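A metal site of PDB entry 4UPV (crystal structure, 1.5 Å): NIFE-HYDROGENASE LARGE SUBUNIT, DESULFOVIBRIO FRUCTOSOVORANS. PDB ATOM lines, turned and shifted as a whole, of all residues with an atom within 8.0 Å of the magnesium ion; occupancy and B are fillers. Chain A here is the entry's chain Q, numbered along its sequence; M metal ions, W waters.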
ATOM      1  N   PHE A  63     -30.641  -3.350  14.680  1.00  0.00           N
ATOM      2  CA  PHE A  63     -29.453  -2.820  15.359  1.00  0.00           C
ATOM      3  C   PHE A  63     -28.261  -2.894  14.416  1.00  0.00           C
ATOM      4  O   PHE A  63     -28.097  -3.895  13.725  1.00  0.00           O
ATOM      5  CB  PHE A  63     -29.150  -3.683  16.606  1.00  0.00           C
ATOM      6  CG  PHE A  63     -27.929  -3.251  17.366  1.00  0.00           C
ATOM      7  CD1 PHE A  63     -28.019  -2.200  18.290  1.00  0.00           C
ATOM      8  CD2 PHE A  63     -26.679  -3.883  17.160  1.00  0.00           C
ATOM      9  CE1 PHE A  63     -26.885  -1.794  19.008  1.00  0.00           C
ATOM     10  CE2 PHE A  63     -25.539  -3.473  17.897  1.00  0.00           C
ATOM     11  CZ  PHE A  63     -25.659  -2.420  18.829  1.00  0.00           C
ATOM     12  N   GLU A  67     -21.692   2.744  17.710  1.00  0.00           N
ATOM     13  CA  GLU A  67     -20.902   3.106  18.890  1.00  0.00           C
ATOM     14  C   GLU A  67     -19.824   2.042  19.152  1.00  0.00           C
ATOM     15  O   GLU A  67     -18.719   2.360  19.522  1.00  0.00           O
ATOM     16  CB  GLU A  67     -21.796   3.280  20.128  1.00  0.00           C
ATOM     17  CG  GLU A  67     -22.772   4.432  19.957  1.00  0.00           C
ATOM     18  CD  GLU A  67     -24.011   4.287  20.805  1.00  0.00           C
ATOM     19  OE1 GLU A  67     -24.375   3.128  21.141  1.00  0.00           O
ATOM     20  OE2 GLU A  67     -24.659   5.334  21.094  1.00  0.00           O
ATOM     21  N   GLU A 348     -29.384   7.372  29.870  1.00  0.00           N
ATOM     22  CA  GLU A 348     -30.162   6.403  29.121  1.00  0.00           C
ATOM     23  C   GLU A 348     -30.313   5.140  29.898  1.00  0.00           C
ATOM     24  O   GLU A 348     -29.356   4.641  30.532  1.00  0.00           O
ATOM     25  CB  GLU A 348     -29.474   6.064  27.774  1.00  0.00           C
ATOM     26  CG  GLU A 348     -29.415   7.263  26.813  1.00  0.00           C
ATOM     27  CD  GLU A 348     -28.671   6.898  25.560  1.00  0.00           C
ATOM     28  OE1 GLU A 348     -27.424   6.693  25.619  1.00  0.00           O
ATOM     29  OE2 GLU A 348     -29.338   6.820  24.493  1.00  0.00           O
ATOM     30  N   TYR A 355     -30.529  -4.913  25.499  1.00  0.00           N
ATOM     31  CA  TYR A 355     -29.166  -4.761  25.990  1.00  0.00           C
ATOM     32  C   TYR A 355     -28.997  -5.543  27.274  1.00  0.00           C
ATOM     33  O   TYR A 355     -29.978  -5.929  27.905  1.00  0.00           O
ATOM     34  CB  TYR A 355     -28.776  -3.274  26.182  1.00  0.00           C
ATOM     35  CG  TYR A 355     -28.826  -2.534  24.859  1.00  0.00           C
ATOM     36  CD1 TYR A 355     -27.795  -2.649  23.919  1.00  0.00           C
ATOM     37  CD2 TYR A 355     -29.953  -1.782  24.519  1.00  0.00           C
ATOM     38  CE1 TYR A 355     -27.875  -2.020  22.667  1.00  0.00           C
ATOM     39  CE2 TYR A 355     -30.043  -1.157  23.281  1.00  0.00           C
ATOM     40  CZ  TYR A 355     -29.015  -1.272  22.373  1.00  0.00           C
ATOM     41  OH  TYR A 355     -29.136  -0.661  21.126  1.00  0.00           O
ATOM     42  N   PRO A 364     -24.276   9.682  29.127  1.00  0.00           N
ATOM     43  CA  PRO A 364     -23.632   9.195  27.904  1.00  0.00           C
ATOM     44  C   PRO A 364     -22.097   9.180  27.906  1.00  0.00           C
ATOM     45  O   PRO A 364     -21.491   8.409  27.178  1.00  0.00           O
ATOM     46  CB  PRO A 364     -24.230  10.094  26.804  1.00  0.00           C
ATOM     47  CG  PRO A 364     -25.488  10.620  27.360  1.00  0.00           C
ATOM     48  CD  PRO A 364     -25.257  10.750  28.846  1.00  0.00           C
ATOM     49  N   GLY A 367     -21.622   5.821  28.808  1.00  0.00           N
ATOM     50  CA  GLY A 367     -22.569   4.918  28.121  1.00  0.00           C
ATOM     51  C   GLY A 367     -21.972   3.546  27.820  1.00  0.00           C
ATOM     52  O   GLY A 367     -20.771   3.381  27.653  1.00  0.00           O
ATOM     53  N   VAL A 368     -22.870   2.571  27.713  1.00  0.00           N
ATOM     54  CA  VAL A 368     -22.530   1.177  27.442  1.00  0.00           C
ATOM     55  C   VAL A 368     -23.509   0.672  26.376  1.00  0.00           C
ATOM     56  O   VAL A 368     -24.725   0.912  26.482  1.00  0.00           O
ATOM     57  CB  VAL A 368     -22.743   0.315  28.707  1.00  0.00           C
ATOM     58  CG1 VAL A 368     -22.338  -1.142  28.448  1.00  0.00           C
ATOM     59  CG2 VAL A 368     -21.977   0.877  29.902  1.00  0.00           C
ATOM     60  N   THR A 369     -22.981  -0.045  25.398  1.00  0.00           N
ATOM     61  CA  THR A 369     -23.791  -0.576  24.296  1.00  0.00           C
ATOM     62  C   THR A 369     -23.457  -2.053  24.147  1.00  0.00           C
ATOM     63  O   THR A 369     -22.519  -2.435  23.430  1.00  0.00           O
ATOM     64  CB  THR A 369     -23.557   0.240  23.011  1.00  0.00           C
ATOM     65  OG1 THR A 369     -23.780   1.626  23.323  1.00  0.00           O
ATOM     66  CG2 THR A 369     -24.526  -0.214  21.944  1.00  0.00           C
ATOM     67  N   TRP A 384     -34.595  -2.177  20.203  1.00  0.00           N
ATOM     68  CA  TRP A 384     -33.179  -1.901  20.073  1.00  0.00           C
ATOM     69  C   TRP A 384     -32.811  -0.457  20.439  1.00  0.00           C
ATOM     70  O   TRP A 384     -31.647  -0.138  20.537  1.00  0.00           O
ATOM     71  CB  TRP A 384     -32.727  -2.203  18.643  1.00  0.00           C
ATOM     72  CG  TRP A 384     -32.593  -3.659  18.360  1.00  0.00           C
ATOM     73  CD1 TRP A 384     -33.350  -4.406  17.492  1.00  0.00           C
ATOM     74  CD2 TRP A 384     -31.620  -4.558  18.921  1.00  0.00           C
ATOM     75  NE1 TRP A 384     -32.905  -5.719  17.481  1.00  0.00           N
ATOM     76  CE2 TRP A 384     -31.840  -5.843  18.334  1.00  0.00           C
ATOM     77  CE3 TRP A 384     -30.585  -4.397  19.850  1.00  0.00           C
ATOM     78  CZ2 TRP A 384     -31.063  -6.971  18.656  1.00  0.00           C
ATOM     79  CZ3 TRP A 384     -29.802  -5.521  20.191  1.00  0.00           C
ATOM     80  CH2 TRP A 384     -30.060  -6.786  19.591  1.00  0.00           C
ATOM     81  N   MET A 385     -33.791   0.435  20.580  1.00  0.00           N
ATOM     82  CA  MET A 385     -33.450   1.775  21.163  1.00  0.00           C
ATOM     83  C   MET A 385     -33.277   1.678  22.664  1.00  0.00           C
ATOM     84  O   MET A 385     -34.005   0.942  23.344  1.00  0.00           O
ATOM     85  CB  MET A 385     -34.531   2.797  20.867  1.00  0.00           C
ATOM     86  CG  MET A 385     -34.637   3.143  19.397  1.00  0.00           C
ATOM     87  SD  MET A 385     -35.610   4.655  19.258  1.00  0.00           S
ATOM     88  CE  MET A 385     -36.053   4.582  17.518  1.00  0.00           C
ATOM     89  N   LYS A 386     -32.293   2.420  23.178  1.00  0.00           N
ATOM     90  CA  LYS A 386     -32.262   2.800  24.596  1.00  0.00           C
ATOM     91  C   LYS A 386     -33.384   3.788  24.902  1.00  0.00           C
ATOM     92  O   LYS A 386     -34.074   4.281  23.997  1.00  0.00           O
ATOM     93  CB  LYS A 386     -30.898   3.397  24.956  1.00  0.00           C
ATOM     94  CG  LYS A 386     -29.726   2.477  24.644  1.00  0.00           C
ATOM     95  CD  LYS A 386     -28.404   3.143  25.079  1.00  0.00           C
ATOM     96  CE  LYS A 386     -27.220   2.230  24.805  1.00  0.00           C
ATOM     97  NZ  LYS A 386     -25.923   3.002  24.846  1.00  0.00           N
ATOM     98  N   PRO A 388     -33.730   7.261  26.612  1.00  0.00           N
ATOM     99  CA  PRO A 388     -33.145   8.448  27.232  1.00  0.00           C
ATOM    100  C   PRO A 388     -34.170   9.124  28.146  1.00  0.00           C
ATOM    101  O   PRO A 388     -35.344   9.227  27.817  1.00  0.00           O
ATOM    102  CB  PRO A 388     -32.797   9.358  26.033  1.00  0.00           C
ATOM    103  CG  PRO A 388     -32.931   8.466  24.810  1.00  0.00           C
ATOM    104  CD  PRO A 388     -34.026   7.499  25.186  1.00  0.00           C
ATOM    105  N   SER A 494     -27.227  14.685  20.517  1.00  0.00           N
ATOM    106  CA  SER A 494     -25.957  14.856  21.193  1.00  0.00           C
ATOM    107  C   SER A 494     -25.038  13.653  20.923  1.00  0.00           C
ATOM    108  O   SER A 494     -25.477  12.510  20.950  1.00  0.00           O
ATOM    109  CB  SER A 494     -26.149  15.131  22.697  1.00  0.00           C
ATOM    110  OG  SER A 494     -26.953  14.150  23.348  1.00  0.00           O
ATOM    111  N   TRP A 496     -21.201  12.167  22.285  1.00  0.00           N
ATOM    112  CA  TRP A 496     -20.346  12.272  23.490  1.00  0.00           C
ATOM    113  C   TRP A 496     -19.149  11.376  23.294  1.00  0.00           C
ATOM    114  O   TRP A 496     -19.310  10.162  23.069  1.00  0.00           O
ATOM    115  CB  TRP A 496     -21.149  11.779  24.701  1.00  0.00           C
ATOM    116  CG  TRP A 496     -22.516  12.411  24.836  1.00  0.00           C
ATOM    117  CD1 TRP A 496     -23.636  12.112  24.128  1.00  0.00           C
ATOM    118  CD2 TRP A 496     -22.900  13.400  25.797  1.00  0.00           C
ATOM    119  NE1 TRP A 496     -24.711  12.871  24.576  1.00  0.00           N
ATOM    120  CE2 TRP A 496     -24.277  13.651  25.621  1.00  0.00           C
ATOM    121  CE3 TRP A 496     -22.207  14.070  26.814  1.00  0.00           C
ATOM    122  CZ2 TRP A 496     -24.968  14.571  26.380  1.00  0.00           C
ATOM    123  CZ3 TRP A 496     -22.917  14.991  27.589  1.00  0.00           C
ATOM    124  CH2 TRP A 496     -24.272  15.241  27.364  1.00  0.00           C
ATOM    125  N   PHE A 507     -17.723   6.359  22.438  1.00  0.00           N
ATOM    126  CA  PHE A 507     -18.424   7.331  21.622  1.00  0.00           C
ATOM    127  C   PHE A 507     -19.886   6.939  21.670  1.00  0.00           C
ATOM    128  O   PHE A 507     -20.248   5.830  21.296  1.00  0.00           O
ATOM    129  CB  PHE A 507     -17.898   7.318  20.181  1.00  0.00           C
ATOM    130  CG  PHE A 507     -18.240   8.555  19.432  1.00  0.00           C
ATOM    131  CD1 PHE A 507     -19.558   8.783  19.020  1.00  0.00           C
ATOM    132  CD2 PHE A 507     -17.269   9.518  19.200  1.00  0.00           C
ATOM    133  CE1 PHE A 507     -19.900   9.946  18.357  1.00  0.00           C
ATOM    134  CE2 PHE A 507     -17.592  10.689  18.510  1.00  0.00           C
ATOM    135  CZ  PHE A 507     -18.923  10.904  18.114  1.00  0.00           C
ATOM    136  N   GLN A 508     -20.715   7.843  22.198  1.00  0.00           N
ATOM    137  CA  GLN A 508     -22.139   7.559  22.405  1.00  0.00           C
ATOM    138  C   GLN A 508     -22.989   8.592  21.698  1.00  0.00           C
ATOM    139  O   GLN A 508     -22.768   9.821  21.817  1.00  0.00           O
ATOM    140  CB  GLN A 508     -22.477   7.542  23.900  1.00  0.00           C
ATOM    141  CG  GLN A 508     -21.775   6.407  24.681  1.00  0.00           C
ATOM    142  CD  GLN A 508     -22.406   5.042  24.424  1.00  0.00           C
ATOM    143  OE1 GLN A 508     -23.614   4.933  24.238  1.00  0.00           O
ATOM    144  NE2 GLN A 508     -21.590   4.003  24.369  1.00  0.00           N
ATOM    145  N   LEU A 509     -23.951   8.098  20.922  1.00  0.00           N
ATOM    146  CA  LEU A 509     -24.977   8.961  20.288  1.00  0.00           C
ATOM    147  C   LEU A 509     -26.252   8.838  21.090  1.00  0.00           C
ATOM    148  O   LEU A 509     -26.684   7.741  21.446  1.00  0.00           O
ATOM    149  CB  LEU A 509     -25.294   8.468  18.849  1.00  0.00           C
ATOM    150  CG  LEU A 509     -24.152   8.531  17.823  1.00  0.00           C
ATOM    151  CD1 LEU A 509     -23.092   7.489  18.065  1.00  0.00           C
ATOM    152  CD2 LEU A 509     -24.726   8.365  16.405  1.00  0.00           C
ATOM    153  N   VAL A 510     -26.876   9.986  21.343  1.00  0.00           N
ATOM    154  CA  VAL A 510     -28.222  10.055  21.921  1.00  0.00           C
ATOM    155  C   VAL A 510     -29.021  10.930  20.950  1.00  0.00           C
ATOM    156  O   VAL A 510     -28.721  12.106  20.790  1.00  0.00           O
ATOM    157  CB  VAL A 510     -28.228  10.658  23.343  1.00  0.00           C
ATOM    158  CG1 VAL A 510     -29.614  10.524  23.969  1.00  0.00           C
ATOM    159  CG2 VAL A 510     -27.183   9.977  24.258  1.00  0.00           C
ATOM    160  N   VAL A 511     -30.021  10.338  20.288  1.00  0.00           N
ATOM    161  CA  VAL A 511     -30.537  10.895  19.054  1.00  0.00           C
ATOM    162  C   VAL A 511     -32.013  11.279  19.266  1.00  0.00           C
ATOM    163  O   VAL A 511     -32.693  10.696  20.116  1.00  0.00           O
ATOM    164  CB  VAL A 511     -30.311   9.859  17.927  1.00  0.00           C
ATOM    165  CG1 VAL A 511     -30.687  10.405  16.557  1.00  0.00           C
ATOM    166  CG2 VAL A 511     -28.824   9.479  17.859  1.00  0.00           C
ATOM    167  N   THR A 514     -34.428   8.563  19.493  1.00  0.00           N
ATOM    168  CA  THR A 514     -34.226   7.779  20.735  1.00  0.00           C
ATOM    169  C   THR A 514     -35.107   8.379  21.831  1.00  0.00           C
ATOM    170  O   THR A 514     -35.847   7.646  22.503  1.00  0.00           O
ATOM    171  CB  THR A 514     -32.733   7.716  21.172  1.00  0.00           C
ATOM    172  OG1 THR A 514     -31.856   7.670  20.012  1.00  0.00           O
ATOM    173  CG2 THR A 514     -32.493   6.484  22.047  1.00  0.00           C
ATOM    174  N   CYS A 560     -31.474   6.372  12.927  1.00  0.00           N
ATOM    175  CA  CYS A 560     -31.041   7.382  13.932  1.00  0.00           C
ATOM    176  C   CYS A 560     -31.196   6.910  15.366  1.00  0.00           C
ATOM    177  O   CYS A 560     -30.285   7.032  16.159  1.00  0.00           O
ATOM    178  CB  CYS A 560     -31.915   8.651  13.794  1.00  0.00           C
ATOM    179  SG  CYS A 560     -31.171   9.923  12.740  1.00  0.00           S
ATOM    180  N   GLY A 561     -32.390   6.400  15.681  1.00  0.00           N
ATOM    181  CA  GLY A 561     -32.721   6.142  17.067  1.00  0.00           C
ATOM    182  C   GLY A 561     -31.876   5.040  17.682  1.00  0.00           C
ATOM    183  O   GLY A 561     -31.505   5.122  18.859  1.00  0.00           O
ATOM    184  N   VAL A 562     -31.572   4.006  16.892  1.00  0.00           N
ATOM    185  CA  VAL A 562     -30.796   2.854  17.399  1.00  0.00           C
ATOM    186  C   VAL A 562     -29.295   2.975  17.101  1.00  0.00           C
ATOM    187  O   VAL A 562     -28.457   2.609  17.938  1.00  0.00           O
ATOM    188  CB  VAL A 562     -31.286   1.538  16.751  1.00  0.00           C
ATOM    189  CG1 VAL A 562     -30.407   0.377  17.239  1.00  0.00           C
ATOM    190  CG2 VAL A 562     -32.748   1.257  17.076  1.00  0.00           C
ATOM    191  N   HIS A 563     -28.966   3.472  15.896  1.00  0.00           N
ATOM    192  CA  HIS A 563     -27.564   3.520  15.450  1.00  0.00           C
ATOM    193  C   HIS A 563     -26.801   2.214  15.744  1.00  0.00           C
ATOM    194  O   HIS A 563     -25.645   2.224  16.175  1.00  0.00           O
ATOM    195  CB  HIS A 563     -26.827   4.794  15.945  1.00  0.00           C
ATOM    196  CG  HIS A 563     -27.130   5.171  17.359  1.00  0.00           C
ATOM    197  ND1 HIS A 563     -28.268   5.859  17.712  1.00  0.00           N
ATOM    198  CD2 HIS A 563     -26.452   4.938  18.508  1.00  0.00           C
ATOM    199  CE1 HIS A 563     -28.280   6.029  19.032  1.00  0.00           C
ATOM    200  NE2 HIS A 563     -27.189   5.477  19.528  1.00  0.00           N
ATOM    201  OXT HIS A 563     -27.373   1.124  15.484  1.00  0.00           O
HETATM  202 MG    MG M   1     -26.694   5.642  21.659  1.00  0.00          MG
HETATM  203  O   HOH W   1     -26.057   5.850  23.612  1.00  0.00           O
HETATM  204  O   HOH W   2     -26.831   3.581  21.926  1.00  0.00           O
HETATM  205  O   HOH W   3     -28.679   5.832  22.177  1.00  0.00           O
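The magnesium ion is bound by water W3, 2.1 Å away. The magnesium ion is bound by water W1. Water W2 is bound to the magnesium ion, 2.1 Å away. The magnesium ion is bound by O of Leu 509. The side-chain carboxylate (OE2) of Glu 67 is bound to the magnesium ion. The magnesium ion is bound by NE2 of His 563 (2.2 Å).
The side-chain amide oxygen of Gln 508 lies close to the side-chain carboxylate of Glu 67. OE1 of Glu 67 sits at hydrogen-bond distance from OG1 of Thr 369 (2.7 Å). ND1 of His 563 is in hydrogen-bond range of O of Cys 560 (2.8 Å).
Water W1 lies within hydrogen-bond range of OE1 of Glu 348 (2.6 Å), OE1 of Gln 508 (2.7 Å) and NZ of Lys 386 (3.1 Å). Water W2 lies within hydrogen-bond range of the side-chain carboxylate of Glu 67 (2.6 Å) and the side-chain amino group of Lys 386 (3.1 Å).
Of the 24 residues printed, 3 come within 4 Å of the magnesium ion. Along chain A the residues within 4 Å of the magnesium ion span positions 67 to 563. The nearest printed residue that does not touch the magnesium ion is Glu 348 (4.1 Å).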
